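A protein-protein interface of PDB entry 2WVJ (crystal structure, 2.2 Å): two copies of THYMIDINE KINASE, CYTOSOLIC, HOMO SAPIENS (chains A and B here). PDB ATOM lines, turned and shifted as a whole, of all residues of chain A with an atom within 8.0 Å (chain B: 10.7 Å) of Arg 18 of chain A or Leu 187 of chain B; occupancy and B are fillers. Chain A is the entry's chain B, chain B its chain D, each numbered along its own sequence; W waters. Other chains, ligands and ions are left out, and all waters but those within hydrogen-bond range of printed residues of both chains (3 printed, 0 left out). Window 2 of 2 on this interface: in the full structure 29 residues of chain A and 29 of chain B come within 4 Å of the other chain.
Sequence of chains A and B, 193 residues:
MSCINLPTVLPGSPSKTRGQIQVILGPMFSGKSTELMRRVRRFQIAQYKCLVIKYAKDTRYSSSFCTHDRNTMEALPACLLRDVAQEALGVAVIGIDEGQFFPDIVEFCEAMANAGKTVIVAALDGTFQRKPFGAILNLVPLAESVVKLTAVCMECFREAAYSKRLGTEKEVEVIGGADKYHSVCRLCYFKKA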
ATOM      1  N   ARG A  18     -17.120  22.868 -27.775  1.00  0.00           N
ATOM      2  CA  ARG A  18     -16.654  21.976 -26.668  1.00  0.00           C
ATOM      3  C   ARG A  18     -15.180  21.560 -26.859  1.00  0.00           C
ATOM      4  O   ARG A  18     -14.861  20.688 -27.676  1.00  0.00           O
ATOM      5  CB  ARG A  18     -17.573  20.759 -26.558  1.00  0.00           C
ATOM      6  CG  ARG A  18     -17.680  20.202 -25.157  1.00  0.00           C
ATOM      7  CD  ARG A  18     -18.743  19.117 -25.049  1.00  0.00           C
ATOM      8  NE  ARG A  18     -18.511  18.318 -23.847  1.00  0.00           N
ATOM      9  CZ  ARG A  18     -19.002  18.597 -22.642  1.00  0.00           C
ATOM     10  NH1 ARG A  18     -19.795  19.646 -22.456  1.00  0.00           N
ATOM     11  NH2 ARG A  18     -18.707  17.814 -21.616  1.00  0.00           N
ATOM     12  N   GLY A  19     -14.293  22.200 -26.100  1.00  0.00           N
ATOM     13  CA  GLY A  19     -12.846  22.060 -26.285  1.00  0.00           C
ATOM     14  C   GLY A  19     -12.169  20.993 -25.448  1.00  0.00           C
ATOM     15  O   GLY A  19     -12.785  20.403 -24.562  1.00  0.00           O
ATOM     16  N   GLN A  20     -10.882  20.775 -25.711  1.00  0.00           N
ATOM     17  CA  GLN A  20     -10.177  19.599 -25.206  1.00  0.00           C
ATOM     18  C   GLN A  20      -8.656  19.734 -25.315  1.00  0.00           C
ATOM     19  O   GLN A  20      -8.154  20.319 -26.272  1.00  0.00           O
ATOM     20  CB  GLN A  20     -10.616  18.387 -26.031  1.00  0.00           C
ATOM     21  CG  GLN A  20     -10.721  17.118 -25.256  1.00  0.00           C
ATOM     22  CD  GLN A  20     -10.441  15.888 -26.094  1.00  0.00           C
ATOM     23  OE1 GLN A  20     -10.697  15.866 -27.297  1.00  0.00           O
ATOM     24  NE2 GLN A  20      -9.914  14.853 -25.454  1.00  0.00           N
ATOM     25  N   ILE A  21      -7.929  19.196 -24.338  1.00  0.00           N
ATOM     26  CA  ILE A  21      -6.477  18.999 -24.474  1.00  0.00           C
ATOM     27  C   ILE A  21      -6.145  17.510 -24.422  1.00  0.00           C
ATOM     28  O   ILE A  21      -6.539  16.802 -23.492  1.00  0.00           O
ATOM     29  CB  ILE A  21      -5.624  19.768 -23.405  1.00  0.00           C
ATOM     30  CG1 ILE A  21      -5.931  21.269 -23.408  1.00  0.00           C
ATOM     31  CG2 ILE A  21      -4.114  19.541 -23.638  1.00  0.00           C
ATOM     32  CD1 ILE A  21      -5.504  21.989 -22.144  1.00  0.00           C
ATOM     33  N   ALA A  92     -10.449  24.732 -35.953  1.00  0.00           N
ATOM     34  CA  ALA A  92     -11.154  23.930 -34.949  1.00  0.00           C
ATOM     35  C   ALA A  92     -10.223  22.998 -34.160  1.00  0.00           C
ATOM     36  O   ALA A  92     -10.464  22.719 -32.987  1.00  0.00           O
ATOM     37  CB  ALA A  92     -12.286  23.142 -35.598  1.00  0.00           C
ATOM     38  N   MET A 112      -6.973  27.898 -25.533  1.00  0.00           N
ATOM     39  CA  MET A 112      -7.550  27.350 -26.762  1.00  0.00           C
ATOM     40  C   MET A 112      -8.647  26.317 -26.505  1.00  0.00           C
ATOM     41  O   MET A 112      -9.680  26.338 -27.178  1.00  0.00           O
ATOM     42  CB  MET A 112      -6.462  26.793 -27.691  1.00  0.00           C
ATOM     43  CG  MET A 112      -5.503  27.851 -28.218  1.00  0.00           C
ATOM     44  SD  MET A 112      -6.322  29.104 -29.236  1.00  0.00           S
ATOM     45  CE  MET A 112      -5.447  30.574 -28.707  1.00  0.00           C
ATOM     46  N   ALA A 113      -8.438  25.439 -25.523  1.00  0.00           N
ATOM     47  CA  ALA A 113      -9.443  24.440 -25.162  1.00  0.00           C
ATOM     48  C   ALA A 113     -10.700  25.074 -24.562  1.00  0.00           C
ATOM     49  O   ALA A 113     -11.811  24.572 -24.769  1.00  0.00           O
ATOM     50  CB  ALA A 113      -8.861  23.396 -24.215  1.00  0.00           C
ATOM     51  N   ASN A 114     -10.527  26.170 -23.825  1.00  0.00           N
ATOM     52  CA  ASN A 114     -11.673  26.892 -23.264  1.00  0.00           C
ATOM     53  C   ASN A 114     -12.443  27.710 -24.306  1.00  0.00           C
ATOM     54  O   ASN A 114     -13.627  27.994 -24.120  1.00  0.00           O
ATOM     55  CB  ASN A 114     -11.261  27.751 -22.059  1.00  0.00           C
ATOM     56  CG  ASN A 114     -10.925  26.912 -20.831  1.00  0.00           C
ATOM     57  OD1 ASN A 114     -11.449  25.807 -20.652  1.00  0.00           O
ATOM     58  ND2 ASN A 114     -10.051  27.434 -19.980  1.00  0.00           N
ATOM     59  N   ALA A 115     -11.771  28.059 -25.406  1.00  0.00           N
ATOM     60  CA  ALA A 115     -12.415  28.692 -26.560  1.00  0.00           C
ATOM     61  C   ALA A 115     -13.040  27.665 -27.518  1.00  0.00           C
ATOM     62  O   ALA A 115     -13.483  28.023 -28.617  1.00  0.00           O
ATOM     63  CB  ALA A 115     -11.427  29.585 -27.302  1.00  0.00           C
ATOM     64  N   GLY A 116     -13.063  26.397 -27.103  1.00  0.00           N
ATOM     65  CA  GLY A 116     -13.753  25.342 -27.847  1.00  0.00           C
ATOM     66  C   GLY A 116     -12.925  24.551 -28.851  1.00  0.00           C
ATOM     67  O   GLY A 116     -13.469  23.737 -29.595  1.00  0.00           O
ATOM     68  N   LYS A 117     -11.613  24.774 -28.874  1.00  0.00           N
ATOM     69  CA  LYS A 117     -10.729  24.048 -29.794  1.00  0.00           C
ATOM     70  C   LYS A 117     -10.294  22.688 -29.241  1.00  0.00           C
ATOM     71  O   LYS A 117     -10.193  22.510 -28.024  1.00  0.00           O
ATOM     72  CB  LYS A 117      -9.490  24.894 -30.128  1.00  0.00           C
ATOM     73  CG  LYS A 117      -9.717  25.981 -31.187  1.00  0.00           C
ATOM     74  CD  LYS A 117     -10.521  27.159 -30.666  1.00  0.00           C
ATOM     75  CE  LYS A 117     -10.583  28.292 -31.689  1.00  0.00           C
ATOM     76  NZ  LYS A 117     -11.549  28.041 -32.800  1.00  0.00           N
ATOM     77  N   THR A 118     -10.045  21.736 -30.143  1.00  0.00           N
ATOM     78  CA  THR A 118      -9.397  20.469 -29.795  1.00  0.00           C
ATOM     79  C   THR A 118      -7.883  20.631 -29.928  1.00  0.00           C
ATOM     80  O   THR A 118      -7.367  20.847 -31.028  1.00  0.00           O
ATOM     81  CB  THR A 118      -9.907  19.292 -30.671  1.00  0.00           C
ATOM     82  OG1 THR A 118     -11.269  19.004 -30.336  1.00  0.00           O
ATOM     83  CG2 THR A 118      -9.069  18.025 -30.443  1.00  0.00           C
ATOM     84  N   VAL A 119      -7.179  20.531 -28.802  1.00  0.00           N
ATOM     85  CA  VAL A 119      -5.728  20.747 -28.771  1.00  0.00           C
ATOM     86  C   VAL A 119      -4.983  19.440 -28.505  1.00  0.00           C
ATOM     87  O   VAL A 119      -5.221  18.764 -27.497  1.00  0.00           O
ATOM     88  CB  VAL A 119      -5.328  21.814 -27.718  1.00  0.00           C
ATOM     89  CG1 VAL A 119      -3.883  22.257 -27.917  1.00  0.00           C
ATOM     90  CG2 VAL A 119      -6.279  23.019 -27.778  1.00  0.00           C
ATOM     91  N   GLU A 144      -7.763  16.211 -20.753  1.00  0.00           N
ATOM     92  CA  GLU A 144      -8.733  15.119 -20.665  1.00  0.00           C
ATOM     93  C   GLU A 144      -8.163  13.782 -21.128  1.00  0.00           C
ATOM     94  O   GLU A 144      -8.642  12.726 -20.733  1.00  0.00           O
ATOM     95  CB  GLU A 144     -10.121  15.449 -21.278  1.00  0.00           C
ATOM     96  CG  GLU A 144     -10.184  16.483 -22.378  1.00  0.00           C
ATOM     97  CD  GLU A 144     -10.133  17.938 -21.890  1.00  0.00           C
ATOM     98  OE1 GLU A 144     -11.193  18.533 -21.579  1.00  0.00           O
ATOM     99  OE2 GLU A 144      -9.019  18.498 -21.868  1.00  0.00           O
ATOM    100  N   ARG B 130      -7.179  21.993 -10.319  1.00  0.00           N
ATOM    101  CA  ARG B 130      -6.543  21.462 -11.532  1.00  0.00           C
ATOM    102  C   ARG B 130      -5.053  21.843 -11.616  1.00  0.00           C
ATOM    103  O   ARG B 130      -4.526  22.160 -12.687  1.00  0.00           O
ATOM    104  CB  ARG B 130      -7.319  21.868 -12.794  1.00  0.00           C
ATOM    105  CG  ARG B 130      -8.771  21.359 -12.860  1.00  0.00           C
ATOM    106  CD  ARG B 130      -9.285  21.413 -14.295  1.00  0.00           C
ATOM    107  NE  ARG B 130      -9.130  22.756 -14.822  1.00  0.00           N
ATOM    108  CZ  ARG B 130      -8.801  23.070 -16.068  1.00  0.00           C
ATOM    109  NH1 ARG B 130      -8.576  22.140 -16.987  1.00  0.00           N
ATOM    110  NH2 ARG B 130      -8.687  24.345 -16.381  1.00  0.00           N
ATOM    111  N   ALA B 151     -13.440   9.383 -15.762  1.00  0.00           N
ATOM    112  CA  ALA B 151     -14.644   9.192 -14.956  1.00  0.00           C
ATOM    113  C   ALA B 151     -15.894   9.601 -15.760  1.00  0.00           C
ATOM    114  O   ALA B 151     -15.785  10.021 -16.916  1.00  0.00           O
ATOM    115  CB  ALA B 151     -14.542  10.008 -13.683  1.00  0.00           C
ATOM    116  N   VAL B 152     -17.071   9.466 -15.151  1.00  0.00           N
ATOM    117  CA  VAL B 152     -18.308  10.037 -15.701  1.00  0.00           C
ATOM    118  C   VAL B 152     -18.564  11.406 -15.048  1.00  0.00           C
ATOM    119  O   VAL B 152     -18.408  11.549 -13.836  1.00  0.00           O
ATOM    120  CB  VAL B 152     -19.532   9.086 -15.488  1.00  0.00           C
ATOM    121  CG1 VAL B 152     -20.825   9.705 -16.036  1.00  0.00           C
ATOM    122  CG2 VAL B 152     -19.284   7.727 -16.143  1.00  0.00           C
ATOM    123  N   CYS B 153     -18.928  12.409 -15.847  1.00  0.00           N
ATOM    124  CA  CYS B 153     -19.289  13.722 -15.300  1.00  0.00           C
ATOM    125  C   CYS B 153     -20.551  13.604 -14.463  1.00  0.00           C
ATOM    126  O   CYS B 153     -21.590  13.158 -14.949  1.00  0.00           O
ATOM    127  CB  CYS B 153     -19.485  14.772 -16.401  1.00  0.00           C
ATOM    128  SG  CYS B 153     -19.864  16.439 -15.768  1.00  0.00           S
ATOM    129  N   MET B 154     -20.454  13.997 -13.198  1.00  0.00           N
ATOM    130  CA  MET B 154     -21.581  13.881 -12.279  1.00  0.00           C
ATOM    131  C   MET B 154     -22.651  14.951 -12.511  1.00  0.00           C
ATOM    132  O   MET B 154     -23.740  14.891 -11.930  1.00  0.00           O
ATOM    133  CB  MET B 154     -21.091  13.886 -10.832  1.00  0.00           C
ATOM    134  CG  MET B 154     -20.502  12.556 -10.417  1.00  0.00           C
ATOM    135  SD  MET B 154     -19.665  12.599  -8.835  1.00  0.00           S
ATOM    136  CE  MET B 154     -19.251  10.866  -8.656  1.00  0.00           C
ATOM    137  N   GLU B 155     -22.348  15.908 -13.385  1.00  0.00           N
ATOM    138  CA  GLU B 155     -23.250  17.032 -13.638  1.00  0.00           C
ATOM    139  C   GLU B 155     -23.888  17.049 -15.039  1.00  0.00           C
ATOM    140  O   GLU B 155     -24.984  17.587 -15.207  1.00  0.00           O
ATOM    141  CB  GLU B 155     -22.555  18.359 -13.291  1.00  0.00           C
ATOM    142  CG  GLU B 155     -22.277  18.499 -11.779  1.00  0.00           C
ATOM    143  CD  GLU B 155     -21.438  19.710 -11.408  1.00  0.00           C
ATOM    144  OE1 GLU B 155     -20.865  19.708 -10.297  1.00  0.00           O
ATOM    145  OE2 GLU B 155     -21.348  20.664 -12.208  1.00  0.00           O
ATOM    146  N   CYS B 156     -23.217  16.461 -16.032  1.00  0.00           N
ATOM    147  CA  CYS B 156     -23.779  16.361 -17.387  1.00  0.00           C
ATOM    148  C   CYS B 156     -23.651  14.955 -17.978  1.00  0.00           C
ATOM    149  O   CYS B 156     -24.170  14.677 -19.063  1.00  0.00           O
ATOM    150  CB  CYS B 156     -23.172  17.405 -18.333  1.00  0.00           C
ATOM    151  SG  CYS B 156     -21.584  16.938 -19.081  1.00  0.00           S
ATOM    152  N   PHE B 157     -22.950  14.084 -17.256  1.00  0.00           N
ATOM    153  CA  PHE B 157     -22.848  12.653 -17.580  1.00  0.00           C
ATOM    154  C   PHE B 157     -22.022  12.310 -18.830  1.00  0.00           C
ATOM    155  O   PHE B 157     -21.996  11.158 -19.263  1.00  0.00           O
ATOM    156  CB  PHE B 157     -24.238  11.989 -17.580  1.00  0.00           C
ATOM    157  CG  PHE B 157     -25.077  12.348 -16.375  1.00  0.00           C
ATOM    158  CD1 PHE B 157     -26.214  13.139 -16.514  1.00  0.00           C
ATOM    159  CD2 PHE B 157     -24.712  11.921 -15.100  1.00  0.00           C
ATOM    160  CE1 PHE B 157     -26.985  13.488 -15.405  1.00  0.00           C
ATOM    161  CE2 PHE B 157     -25.474  12.263 -13.982  1.00  0.00           C
ATOM    162  CZ  PHE B 157     -26.614  13.047 -14.134  1.00  0.00           C
ATOM    163  N   ARG B 158     -21.329  13.305 -19.390  1.00  0.00           N
ATOM    164  CA  ARG B 158     -20.276  13.043 -20.374  1.00  0.00           C
ATOM    165  C   ARG B 158     -19.002  12.555 -19.654  1.00  0.00           C
ATOM    166  O   ARG B 158     -19.046  12.218 -18.464  1.00  0.00           O
ATOM    167  CB  ARG B 158     -20.026  14.276 -21.252  1.00  0.00           C
ATOM    168  CG  ARG B 158     -21.205  14.590 -22.181  1.00  0.00           C
ATOM    169  CD  ARG B 158     -20.979  15.824 -23.045  1.00  0.00           C
ATOM    170  NE  ARG B 158     -20.254  15.529 -24.286  1.00  0.00           N
ATOM    171  CZ  ARG B 158     -20.825  15.215 -25.451  1.00  0.00           C
ATOM    172  NH1 ARG B 158     -22.150  15.139 -25.566  1.00  0.00           N
ATOM    173  NH2 ARG B 158     -20.063  14.966 -26.510  1.00  0.00           N
ATOM    174  N   GLU B 159     -17.880  12.490 -20.364  1.00  0.00           N
ATOM    175  CA  GLU B 159     -16.623  12.039 -19.750  1.00  0.00           C
ATOM    176  C   GLU B 159     -16.004  13.111 -18.855  1.00  0.00           C
ATOM    177  O   GLU B 159     -15.989  14.289 -19.211  1.00  0.00           O
ATOM    178  CB  GLU B 159     -15.614  11.590 -20.807  1.00  0.00           C
ATOM    179  CG  GLU B 159     -15.988  10.296 -21.492  1.00  0.00           C
ATOM    180  CD  GLU B 159     -14.789   9.555 -22.064  1.00  0.00           C
ATOM    181  OE1 GLU B 159     -13.849  10.212 -22.573  1.00  0.00           O
ATOM    182  OE2 GLU B 159     -14.802   8.306 -22.012  1.00  0.00           O
ATOM    183  N   ALA B 160     -15.489  12.681 -17.704  1.00  0.00           N
ATOM    184  CA  ALA B 160     -14.908  13.576 -16.699  1.00  0.00           C
ATOM    185  C   ALA B 160     -13.399  13.381 -16.524  1.00  0.00           C
ATOM    186  O   ALA B 160     -12.925  12.254 -16.387  1.00  0.00           O
ATOM    187  CB  ALA B 160     -15.612  13.382 -15.367  1.00  0.00           C
ATOM    188  N   ALA B 161     -12.665  14.491 -16.500  1.00  0.00           N
ATOM    189  CA  ALA B 161     -11.202  14.489 -16.369  1.00  0.00           C
ATOM    190  C   ALA B 161     -10.696  15.190 -15.103  1.00  0.00           C
ATOM    191  O   ALA B 161      -9.487  15.179 -14.821  1.00  0.00           O
ATOM    192  CB  ALA B 161     -10.573  15.135 -17.596  1.00  0.00           C
ATOM    193  N   TYR B 162     -11.617  15.797 -14.353  1.00  0.00           N
ATOM    194  CA  TYR B 162     -11.267  16.701 -13.250  1.00  0.00           C
ATOM    195  C   TYR B 162     -12.063  16.403 -11.994  1.00  0.00           C
ATOM    196  O   TYR B 162     -13.106  15.749 -12.052  1.00  0.00           O
ATOM    197  CB  TYR B 162     -11.469  18.170 -13.679  1.00  0.00           C
ATOM    198  CG  TYR B 162     -10.956  18.433 -15.076  1.00  0.00           C
ATOM    199  CD1 TYR B 162     -11.830  18.736 -16.118  1.00  0.00           C
ATOM    200  CD2 TYR B 162      -9.593  18.325 -15.366  1.00  0.00           C
ATOM    201  CE1 TYR B 162     -11.356  18.945 -17.412  1.00  0.00           C
ATOM    202  CE2 TYR B 162      -9.111  18.526 -16.653  1.00  0.00           C
ATOM    203  CZ  TYR B 162      -9.994  18.838 -17.667  1.00  0.00           C
ATOM    204  OH  TYR B 162      -9.508  19.036 -18.933  1.00  0.00           O
ATOM    205  N   LYS B 164     -13.935  18.349  -8.903  1.00  0.00           N
ATOM    206  CA  LYS B 164     -14.462  19.635  -8.480  1.00  0.00           C
ATOM    207  C   LYS B 164     -14.885  19.598  -7.016  1.00  0.00           C
ATOM    208  O   LYS B 164     -15.734  18.795  -6.628  1.00  0.00           O
ATOM    209  CB  LYS B 164     -15.624  20.051  -9.385  1.00  0.00           C
ATOM    210  CG  LYS B 164     -16.407  21.274  -8.914  1.00  0.00           C
ATOM    211  CD  LYS B 164     -17.107  21.929 -10.090  1.00  0.00           C
ATOM    212  CE  LYS B 164     -18.529  22.324  -9.758  1.00  0.00           C
ATOM    213  NZ  LYS B 164     -19.187  22.958 -10.944  1.00  0.00           N
ATOM    214  N   SER B 183     -16.636  14.334  -9.872  1.00  0.00           N
ATOM    215  CA  SER B 183     -15.890  14.168 -11.117  1.00  0.00           C
ATOM    216  C   SER B 183     -16.642  14.966 -12.174  1.00  0.00           C
ATOM    217  O   SER B 183     -17.875  14.967 -12.206  1.00  0.00           O
ATOM    218  CB  SER B 183     -15.760  12.698 -11.528  1.00  0.00           C
ATOM    219  OG  SER B 183     -17.018  12.052 -11.575  1.00  0.00           O
ATOM    220  N   VAL B 184     -15.892  15.638 -13.037  1.00  0.00           N
ATOM    221  CA  VAL B 184     -16.443  16.707 -13.846  1.00  0.00           C
ATOM    222  C   VAL B 184     -15.690  16.876 -15.182  1.00  0.00           C
ATOM    223  O   VAL B 184     -14.472  16.660 -15.254  1.00  0.00           O
ATOM    224  CB  VAL B 184     -16.493  18.001 -12.961  1.00  0.00           C
ATOM    225  CG1 VAL B 184     -15.595  19.103 -13.461  1.00  0.00           C
ATOM    226  CG2 VAL B 184     -17.929  18.449 -12.688  1.00  0.00           C
ATOM    227  N   CYS B 185     -16.427  17.219 -16.238  1.00  0.00           N
ATOM    228  CA  CYS B 185     -15.821  17.607 -17.512  1.00  0.00           C
ATOM    229  C   CYS B 185     -15.374  19.065 -17.440  1.00  0.00           C
ATOM    230  O   CYS B 185     -15.624  19.744 -16.444  1.00  0.00           O
ATOM    231  CB  CYS B 185     -16.816  17.427 -18.661  1.00  0.00           C
ATOM    232  SG  CYS B 185     -18.165  18.641 -18.662  1.00  0.00           S
ATOM    233  N   ARG B 186     -14.733  19.544 -18.504  1.00  0.00           N
ATOM    234  CA  ARG B 186     -14.245  20.923 -18.594  1.00  0.00           C
ATOM    235  C   ARG B 186     -15.340  21.979 -18.405  1.00  0.00           C
ATOM    236  O   ARG B 186     -15.173  22.912 -17.615  1.00  0.00           O
ATOM    237  CB  ARG B 186     -13.530  21.135 -19.935  1.00  0.00           C
ATOM    238  CG  ARG B 186     -12.973  22.530 -20.177  1.00  0.00           C
ATOM    239  CD  ARG B 186     -12.214  22.585 -21.503  1.00  0.00           C
ATOM    240  NE  ARG B 186     -11.036  21.720 -21.466  1.00  0.00           N
ATOM    241  CZ  ARG B 186      -9.823  22.106 -21.078  1.00  0.00           C
ATOM    242  NH1 ARG B 186      -9.604  23.362 -20.710  1.00  0.00           N
ATOM    243  NH2 ARG B 186      -8.824  21.231 -21.069  1.00  0.00           N
ATOM    244  N   LEU B 187     -16.447  21.833 -19.135  1.00  0.00           N
ATOM    245  CA  LEU B 187     -17.528  22.819 -19.091  1.00  0.00           C
ATOM    246  C   LEU B 187     -18.166  22.901 -17.711  1.00  0.00           C
ATOM    247  O   LEU B 187     -18.433  24.000 -17.214  1.00  0.00           O
ATOM    248  CB  LEU B 187     -18.598  22.540 -20.158  1.00  0.00           C
ATOM    249  CG  LEU B 187     -18.265  22.754 -21.641  1.00  0.00           C
ATOM    250  CD1 LEU B 187     -19.550  22.717 -22.451  1.00  0.00           C
ATOM    251  CD2 LEU B 187     -17.525  24.062 -21.898  1.00  0.00           C
ATOM    252  N   CYS B 188     -18.388  21.742 -17.094  1.00  0.00           N
ATOM    253  CA  CYS B 188     -18.996  21.678 -15.770  1.00  0.00           C
ATOM    254  C   CYS B 188     -18.063  22.133 -14.660  1.00  0.00           C
ATOM    255  O   CYS B 188     -18.538  22.569 -13.610  1.00  0.00           O
ATOM    256  CB  CYS B 188     -19.533  20.279 -15.478  1.00  0.00           C
ATOM    257  SG  CYS B 188     -20.933  19.831 -16.515  1.00  0.00           S
ATOM    258  N   TYR B 189     -16.750  22.029 -14.890  1.00  0.00           N
ATOM    259  CA  TYR B 189     -15.755  22.539 -13.942  1.00  0.00           C
ATOM    260  C   TYR B 189     -15.884  24.047 -13.743  1.00  0.00           C
ATOM    261  O   TYR B 189     -15.802  24.533 -12.617  1.00  0.00           O
ATOM    262  CB  TYR B 189     -14.314  22.193 -14.367  1.00  0.00           C
ATOM    263  CG  TYR B 189     -13.277  22.661 -13.361  1.00  0.00           C
ATOM    264  CD1 TYR B 189     -12.948  21.878 -12.252  1.00  0.00           C
ATOM    265  CD2 TYR B 189     -12.650  23.904 -13.496  1.00  0.00           C
ATOM    266  CE1 TYR B 189     -12.014  22.309 -11.315  1.00  0.00           C
ATOM    267  CE2 TYR B 189     -11.715  24.345 -12.564  1.00  0.00           C
ATOM    268  CZ  TYR B 189     -11.401  23.543 -11.477  1.00  0.00           C
ATOM    269  OH  TYR B 189     -10.474  23.969 -10.558  1.00  0.00           O
ATOM    270  N   PHE B 190     -16.081  24.765 -14.847  1.00  0.00           N
ATOM    271  CA  PHE B 190     -16.087  26.227 -14.853  1.00  0.00           C
ATOM    272  C   PHE B 190     -17.467  26.865 -14.638  1.00  0.00           C
ATOM    273  O   PHE B 190     -17.609  28.085 -14.758  1.00  0.00           O
ATOM    274  CB  PHE B 190     -15.469  26.753 -16.157  1.00  0.00           C
ATOM    275  CG  PHE B 190     -13.971  26.608 -16.231  1.00  0.00           C
ATOM    276  CD1 PHE B 190     -13.390  25.743 -17.154  1.00  0.00           C
ATOM    277  CD2 PHE B 190     -13.145  27.344 -15.389  1.00  0.00           C
ATOM    278  CE1 PHE B 190     -12.008  25.612 -17.236  1.00  0.00           C
ATOM    279  CE2 PHE B 190     -11.756  27.219 -15.459  1.00  0.00           C
ATOM    280  CZ  PHE B 190     -11.187  26.354 -16.386  1.00  0.00           C
ATOM    281  N   LYS B 191     -18.475  26.050 -14.324  1.00  0.00           N
ATOM    282  CA  LYS B 191     -19.822  26.562 -14.054  1.00  0.00           C
ATOM    283  C   LYS B 191     -19.928  27.172 -12.660  1.00  0.00           C
ATOM    284  O   LYS B 191     -19.627  26.521 -11.654  1.00  0.00           O
ATOM    285  CB  LYS B 191     -20.872  25.466 -14.229  1.00  0.00           C
ATOM    286  CG  LYS B 191     -21.361  25.302 -15.656  1.00  0.00           C
ATOM    287  CD  LYS B 191     -22.675  24.533 -15.708  1.00  0.00           C
ATOM    288  CE  LYS B 191     -23.862  25.388 -15.260  1.00  0.00           C
ATOM    289  NZ  LYS B 191     -25.141  24.611 -15.283  1.00  0.00           N
HETATM  290  O   HOH W   1     -16.645  15.368 -21.938  1.00  0.00           O
HETATM  291  O   HOH W   2     -16.120  19.746 -21.727  1.00  0.00           O
HETATM  292  O   HOH W   3     -13.805  18.013 -20.764  1.00  0.00           O
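The guanidinium group of Arg 18 of chain A lies close to the side-chain sulfur of Cys 185 of chain B (3.1 Å). OD1 of Asn 114 of chain A lies within hydrogen-bond range of NH1 of Arg 186 of chain B (3.1 Å). The side-chain carboxylate of Glu 144 of chain A lies within hydrogen-bond range of the side-chain hydroxyl of Tyr 162 of chain B, at 3.0 Å. The side-chain carboxylate (OE2) of Glu 144 of chain A lies within salt-bridge range of the guanidinium group (NH2) of Arg 186 of chain B, at 2.9 Å. The guanidinium group (NE) of Arg 18 of chain A sits close to the guanidinium group (NE) of Arg 158 of chain B, 3.3 Å away.
The backbone NH (N) of Ile 21 of chain A sits at hydrogen-bond distance from the side-chain carboxylate (OE2) of Glu 144 of chain A (2.8 Å). The backbone NH of Cys 153 of chain B lies within hydrogen-bond range of the backbone carbonyl oxygen of Arg 158 of chain B, at 2.6 Å. N of Ala 161 of chain B sits at hydrogen-bond distance from O of Val 184 of chain B (3.1 Å). The backbone carbonyl oxygen of Tyr 162 of chain B sits at hydrogen-bond distance from the backbone NH of Val 184 of chain B (3.0 Å). The side-chain hydroxyl (OH) of Tyr 162 of chain B lies within hydrogen-bond range of the guanidinium group (NH2) of Arg 186 of chain B, 3.1 Å away. The side-chain sulfur (SG) of Cys 185 of chain B lies close to the backbone NH (N) of Leu 187 of chain B, 3.7 Å away.
Among the printed residues, pairs that only touch across the chains: Arg 18 of chain A with Leu 187 of chain B, Asn 114 of chain A with Phe 190 of chain B, Ala 113 of chain A with Arg 186 of chain B, Ile 21 of chain A with Arg 186 of chain B, Glu 144 of chain A with Ala 161 of chain B, Gly 19 of chain A with Arg 186 of chain B and Arg 18 of chain A with Cys 156 of chain B.
Arg 18 of chain A touches just these residues of chain B: Cys 156 (3.9 Å), Arg 158 (3.3 Å), Cys 185 (3.1 Å) and Leu 187 (3.1 Å). Leu 187 of chain B touches just one residue of chain A: Arg 18 (3.1 Å). Gly 19 of chain A touches just one residue of chain B: Arg 186. No residue of chain B comes within 4 Å of Gly 116 of chain A. Printed residues of chain A within 4 Å of Cys 185 of chain B: Arg 18 (3.1 Å). Of the printed residues of chain A, Ala 161 of chain B touches Glu 144. Of the printed residues of chain B, Asn 114 of chain A touches Arg 186 and Phe 190. Of the printed residues of chain A, Arg 186 of chain B touches Gly 19 (3.8 Å), Ile 21 (3.6 Å), Ala 113 (3.5 Å), Asn 114 (3.1 Å) and Glu 144 (2.9 Å). Met 154 of chain B touches none of the printed residues of chain A. Phe 157 of chain B touches none of the printed residues of chain A. The nearest residue of chain A that does not touch Leu 187 of chain B is Gly 19 of chain A (5.6 Å). The nearest printed residue of chain B that does not touch Ala 113 of chain A is Leu 187 of chain B (6.4 Å).
Of the 23 printed residues of chain B, 8 touch a printed residue of chain A. Among the printed residues, 12 pairs touch across the chains. Among the printed residues, Asp or Glu carboxylates within 4 Å of a Lys or Arg side-chain nitrogen of the other chain: Glu 144 of chain A with Arg 186 of chain B.
No position is printed for both chains. Of the 12 pairs that touch across the chains among the printed residues, none has its exchanged pair printed and touching as well.
Water W3 bridges OE1 of Glu 144 of chain A (2.8 Å) and N of Arg 186 of chain B (2.9 Å). Water W1 bridges the backbone carbonyl oxygen (O) of Glu 159 of chain B (3.0 Å) and the guanidinium group (NH2) of Arg 18 of chain A (3.2 Å). Water W2 lies within hydrogen-bond range of NH2 of Arg 18 of chain A (3.2 Å) and N of Leu 187 of chain B (3.3 Å).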
